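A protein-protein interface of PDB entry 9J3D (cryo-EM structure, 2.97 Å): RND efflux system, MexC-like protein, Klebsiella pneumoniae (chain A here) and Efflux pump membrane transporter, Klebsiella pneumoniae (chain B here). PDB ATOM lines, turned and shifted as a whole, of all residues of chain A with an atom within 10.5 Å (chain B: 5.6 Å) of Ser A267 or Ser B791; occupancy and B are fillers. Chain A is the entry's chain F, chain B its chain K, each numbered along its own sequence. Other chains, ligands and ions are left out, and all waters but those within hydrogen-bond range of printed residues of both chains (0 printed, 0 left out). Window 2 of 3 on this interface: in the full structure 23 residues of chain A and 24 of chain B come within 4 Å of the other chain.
Of the 11 printed residues of chain A, 3 touch a printed residue of chain B. Printed residues of chain A that touch a printed residue of chain B: Arg A266, Ser A267 and Thr A268. Of the 7 printed residues of chain B, 5 touch a printed residue of chain A. Printed residues of chain B that touch a printed residue of chain A: Leu B735, Asn B789, Ser B791, Ser B793 and Val B795. Along chain B the printed residues that touch a printed residue of chain A span positions 735 to 795.
Leu B735 touches Arg A266. O of Ser A267 touches O of Leu B735 (3.8 Å). Ser A267 touches Ser B791 (OG to OG, 3.7 Å). Ser A267 touches Ser B793. O of Ser A267 touches CG2 of Val B795, 3.5 Å away. CG2 of Thr A268 touches CB of Ser B793, 3.8 Å away. Thr A268 touches Val B795 (O to CG1, 3.3 Å).
OD1 of Asp A265 lies within hydrogen-bond range of N of Ser A267 (2.9 Å). The backbone NH (N) of Thr A268 lies within hydrogen-bond range of the side-chain carboxylate (OD1) of Asp A265 (2.8 Å). The side-chain amide nitrogen (ND2) of Asn B789 lies within hydrogen-bond range of the side-chain hydroxyl (OG) of Ser B791 (3.0 Å). N of Gly B792 is in hydrogen-bond range of OD1 of Asn B789 (2.9 Å). The backbone NH (N) of Ser B793 sits at hydrogen-bond distance from the side-chain amide oxygen (OD1) of Asn B789, 2.6 Å away.
Of the printed residues of chain B, Arg A266 touches Leu B735 (3.5 Å). Of the printed residues of chain B, Ser A267 touches Leu B735, Asn B789, Ser B791, Ser B793 and Val B795. Of the printed residues of chain B, Thr A268 touches Ser B793 (3.8 Å) and Val B795 (3.3 Å). Printed residues of chain A within 4 Å of Ser B791: Ser A267 (3.7 Å). No residue of chain A comes within 4 Å of Gly B792. Printed residues of chain A within 4 Å of Val B795: Ser A267 (3.5 Å) and Thr A268 (3.3 Å). The nearest printed residue of chain B that does not touch Ser A267 is Gly B792 (6.4 Å). The nearest residue of chain A that does not touch Ser B791 is Thr A268 (6.7 Å).
The side-chain amide nitrogen of Asn B789 sits at hydrogen-bond distance from the side-chain hydroxyl of Ser A267 (2.9 Å).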
ATOM      1  N   THR A 216      17.241 -19.324 -17.547  1.00  0.00           N
ATOM      2  CA  THR A 216      15.938 -19.107 -16.938  1.00  0.00           C
ATOM      3  C   THR A 216      14.813 -19.647 -17.814  1.00  0.00           C
ATOM      4  O   THR A 216      14.844 -19.520 -19.041  1.00  0.00           O
ATOM      5  CB  THR A 216      15.742 -17.618 -16.652  1.00  0.00           C
ATOM      6  OG1 THR A 216      16.790 -17.169 -15.784  1.00  0.00           O
ATOM      7  CG2 THR A 216      14.449 -17.390 -15.937  1.00  0.00           C
ATOM      8  N   ALA A 219       7.742 -20.307 -15.730  1.00  0.00           N
ATOM      9  CA  ALA A 219       7.182 -21.216 -14.734  1.00  0.00           C
ATOM     10  C   ALA A 219       6.093 -22.107 -15.318  1.00  0.00           C
ATOM     11  O   ALA A 219       5.998 -23.286 -14.954  1.00  0.00           O
ATOM     12  CB  ALA A 219       6.634 -20.420 -13.551  1.00  0.00           C
ATOM     13  N   SER A 263      11.747 -21.474  -6.190  1.00  0.00           N
ATOM     14  CA  SER A 263      11.042 -20.209  -6.057  1.00  0.00           C
ATOM     15  C   SER A 263      10.922 -19.533  -7.415  1.00  0.00           C
ATOM     16  O   SER A 263      11.875 -19.513  -8.199  1.00  0.00           O
ATOM     17  CB  SER A 263      11.763 -19.283  -5.077  1.00  0.00           C
ATOM     18  OG  SER A 263      12.999 -18.841  -5.610  1.00  0.00           O
ATOM     19  N   VAL A 264       9.746 -18.980  -7.686  1.00  0.00           N
ATOM     20  CA  VAL A 264       9.459 -18.300  -8.941  1.00  0.00           C
ATOM     21  C   VAL A 264       9.709 -16.813  -8.753  1.00  0.00           C
ATOM     22  O   VAL A 264       9.214 -16.211  -7.791  1.00  0.00           O
ATOM     23  CB  VAL A 264       8.013 -18.559  -9.394  1.00  0.00           C
ATOM     24  CG1 VAL A 264       7.728 -17.835 -10.693  1.00  0.00           C
ATOM     25  CG2 VAL A 264       7.767 -20.048  -9.540  1.00  0.00           C
ATOM     26  N   ASP A 265      10.478 -16.220  -9.661  1.00  0.00           N
ATOM     27  CA  ASP A 265      10.756 -14.791  -9.592  1.00  0.00           C
ATOM     28  C   ASP A 265       9.463 -14.003  -9.747  1.00  0.00           C
ATOM     29  O   ASP A 265       8.764 -14.133 -10.755  1.00  0.00           O
ATOM     30  CB  ASP A 265      11.761 -14.399 -10.673  1.00  0.00           C
ATOM     31  CG  ASP A 265      12.134 -12.932 -10.619  1.00  0.00           C
ATOM     32  OD1 ASP A 265      11.325 -12.091 -11.063  1.00  0.00           O
ATOM     33  OD2 ASP A 265      13.241 -12.617 -10.136  1.00  0.00           O
ATOM     34  N   ARG A 266       9.147 -13.184  -8.743  1.00  0.00           N
ATOM     35  CA  ARG A 266       7.883 -12.458  -8.734  1.00  0.00           C
ATOM     36  C   ARG A 266       7.785 -11.439  -9.861  1.00  0.00           C
ATOM     37  O   ARG A 266       6.692 -11.227 -10.393  1.00  0.00           O
ATOM     38  CB  ARG A 266       7.693 -11.761  -7.388  1.00  0.00           C
ATOM     39  CG  ARG A 266       6.294 -11.878  -6.819  1.00  0.00           C
ATOM     40  CD  ARG A 266       6.258 -11.421  -5.372  1.00  0.00           C
ATOM     41  NE  ARG A 266       6.368 -12.540  -4.447  1.00  0.00           N
ATOM     42  CZ  ARG A 266       5.498 -12.803  -3.482  1.00  0.00           C
ATOM     43  NH1 ARG A 266       4.439 -12.037  -3.279  1.00  0.00           N
ATOM     44  NH2 ARG A 266       5.697 -13.860  -2.699  1.00  0.00           N
ATOM     45  N   SER A 267       8.895 -10.800 -10.228  1.00  0.00           N
ATOM     46  CA  SER A 267       8.853  -9.781 -11.269  1.00  0.00           C
ATOM     47  C   SER A 267       8.660 -10.377 -12.656  1.00  0.00           C
ATOM     48  O   SER A 267       7.973  -9.780 -13.489  1.00  0.00           O
ATOM     49  CB  SER A 267      10.131  -8.943 -11.233  1.00  0.00           C
ATOM     50  OG  SER A 267      10.483  -8.488 -12.528  1.00  0.00           O
ATOM     51  N   THR A 268       9.253 -11.541 -12.926  1.00  0.00           N
ATOM     52  CA  THR A 268       9.219 -12.128 -14.256  1.00  0.00           C
ATOM     53  C   THR A 268       8.388 -13.396 -14.357  1.00  0.00           C
ATOM     54  O   THR A 268       8.105 -13.836 -15.475  1.00  0.00           O
ATOM     55  CB  THR A 268      10.642 -12.441 -14.739  1.00  0.00           C
ATOM     56  OG1 THR A 268      11.225 -13.435 -13.889  1.00  0.00           O
ATOM     57  CG2 THR A 268      11.502 -11.191 -14.709  1.00  0.00           C
ATOM     58  N   GLY A 269       7.992 -13.991 -13.236  1.00  0.00           N
ATOM     59  CA  GLY A 269       7.252 -15.234 -13.295  1.00  0.00           C
ATOM     60  C   GLY A 269       8.028 -16.395 -13.865  1.00  0.00           C
ATOM     61  O   GLY A 269       7.429 -17.298 -14.453  1.00  0.00           O
ATOM     62  N   GLN A 270       9.344 -16.406 -13.699  1.00  0.00           N
ATOM     63  CA  GLN A 270      10.199 -17.444 -14.249  1.00  0.00           C
ATOM     64  C   GLN A 270      11.016 -18.089 -13.137  1.00  0.00           C
ATOM     65  O   GLN A 270      11.246 -17.488 -12.084  1.00  0.00           O
ATOM     66  CB  GLN A 270      11.147 -16.876 -15.306  1.00  0.00           C
ATOM     67  CG  GLN A 270      10.560 -15.810 -16.212  1.00  0.00           C
ATOM     68  CD  GLN A 270      11.562 -15.307 -17.243  1.00  0.00           C
ATOM     69  OE1 GLN A 270      12.331 -16.083 -17.805  1.00  0.00           O
ATOM     70  NE2 GLN A 270      11.568 -14.003 -17.476  1.00  0.00           N
ATOM     71  N   ILE A 271      11.454 -19.318 -13.380  1.00  0.00           N
ATOM     72  CA  ILE A 271      12.320 -20.038 -12.457  1.00  0.00           C
ATOM     73  C   ILE A 271      13.734 -20.058 -13.016  1.00  0.00           C
ATOM     74  O   ILE A 271      13.943 -20.122 -14.236  1.00  0.00           O
ATOM     75  CB  ILE A 271      11.799 -21.465 -12.203  1.00  0.00           C
ATOM     76  CG1 ILE A 271      11.848 -22.298 -13.480  1.00  0.00           C
ATOM     77  CG2 ILE A 271      10.387 -21.425 -11.664  1.00  0.00           C
ATOM     78  CD1 ILE A 271      11.676 -23.777 -13.241  1.00  0.00           C
ATOM     79  N   LEU B 735       2.136  -8.679 -13.107  1.00  0.00           N
ATOM     80  CA  LEU B 735       3.551  -8.721 -13.443  1.00  0.00           C
ATOM     81  C   LEU B 735       4.078  -7.383 -13.947  1.00  0.00           C
ATOM     82  O   LEU B 735       5.242  -7.309 -14.351  1.00  0.00           O
ATOM     83  CB  LEU B 735       3.807  -9.806 -14.489  1.00  0.00           C
ATOM     84  CG  LEU B 735       3.483 -11.234 -14.053  1.00  0.00           C
ATOM     85  CD1 LEU B 735       3.488 -12.177 -15.238  1.00  0.00           C
ATOM     86  CD2 LEU B 735       4.463 -11.701 -12.999  1.00  0.00           C
ATOM     87  N   ASN B 789       8.454  -5.077 -18.155  1.00  0.00           N
ATOM     88  CA  ASN B 789       7.532  -4.716 -17.092  1.00  0.00           C
ATOM     89  C   ASN B 789       7.857  -3.315 -16.582  1.00  0.00           C
ATOM     90  O   ASN B 789       8.731  -2.622 -17.106  1.00  0.00           O
ATOM     91  CB  ASN B 789       7.572  -5.753 -15.967  1.00  0.00           C
ATOM     92  CG  ASN B 789       8.921  -5.832 -15.283  1.00  0.00           C
ATOM     93  OD1 ASN B 789       9.868  -5.141 -15.653  1.00  0.00           O
ATOM     94  ND2 ASN B 789       9.013  -6.684 -14.273  1.00  0.00           N
ATOM     95  N   ASP B 790       7.139  -2.893 -15.539  1.00  0.00           N
ATOM     96  CA  ASP B 790       7.360  -1.559 -14.991  1.00  0.00           C
ATOM     97  C   ASP B 790       8.727  -1.414 -14.335  1.00  0.00           C
ATOM     98  O   ASP B 790       9.251  -0.299 -14.259  1.00  0.00           O
ATOM     99  CB  ASP B 790       6.245  -1.205 -13.999  1.00  0.00           C
ATOM    100  CG  ASP B 790       6.309  -2.015 -12.711  1.00  0.00           C
ATOM    101  OD1 ASP B 790       5.480  -1.752 -11.815  1.00  0.00           O
ATOM    102  OD2 ASP B 790       7.151  -2.929 -12.595  1.00  0.00           O
ATOM    103  N   SER B 791       9.316  -2.510 -13.865  1.00  0.00           N
ATOM    104  CA  SER B 791      10.611  -2.476 -13.203  1.00  0.00           C
ATOM    105  C   SER B 791      11.778  -2.669 -14.161  1.00  0.00           C
ATOM    106  O   SER B 791      12.927  -2.716 -13.711  1.00  0.00           O
ATOM    107  CB  SER B 791      10.669  -3.542 -12.106  1.00  0.00           C
ATOM    108  OG  SER B 791      10.793  -4.837 -12.665  1.00  0.00           O
ATOM    109  N   GLY B 792      11.517  -2.785 -15.460  1.00  0.00           N
ATOM    110  CA  GLY B 792      12.577  -2.949 -16.432  1.00  0.00           C
ATOM    111  C   GLY B 792      13.005  -4.374 -16.697  1.00  0.00           C
ATOM    112  O   GLY B 792      13.903  -4.589 -17.517  1.00  0.00           O
ATOM    113  N   SER B 793      12.403  -5.353 -16.029  1.00  0.00           N
ATOM    114  CA  SER B 793      12.726  -6.748 -16.287  1.00  0.00           C
ATOM    115  C   SER B 793      11.850  -7.289 -17.408  1.00  0.00           C
ATOM    116  O   SER B 793      10.757  -6.778 -17.664  1.00  0.00           O
ATOM    117  CB  SER B 793      12.539  -7.584 -15.023  1.00  0.00           C
ATOM    118  OG  SER B 793      13.408  -7.150 -13.993  1.00  0.00           O
ATOM    119  N   VAL B 795       9.575 -10.181 -19.171  1.00  0.00           N
ATOM    120  CA  VAL B 795       8.661 -11.256 -18.813  1.00  0.00           C
ATOM    121  C   VAL B 795       8.291 -11.987 -20.096  1.00  0.00           C
ATOM    122  O   VAL B 795       7.892 -11.343 -21.066  1.00  0.00           O
ATOM    123  CB  VAL B 795       7.392 -10.734 -18.116  1.00  0.00           C
ATOM    124  CG1 VAL B 795       6.571 -11.883 -17.575  1.00  0.00           C
ATOM    125  CG2 VAL B 795       7.758  -9.761 -17.010  1.00  0.00           C
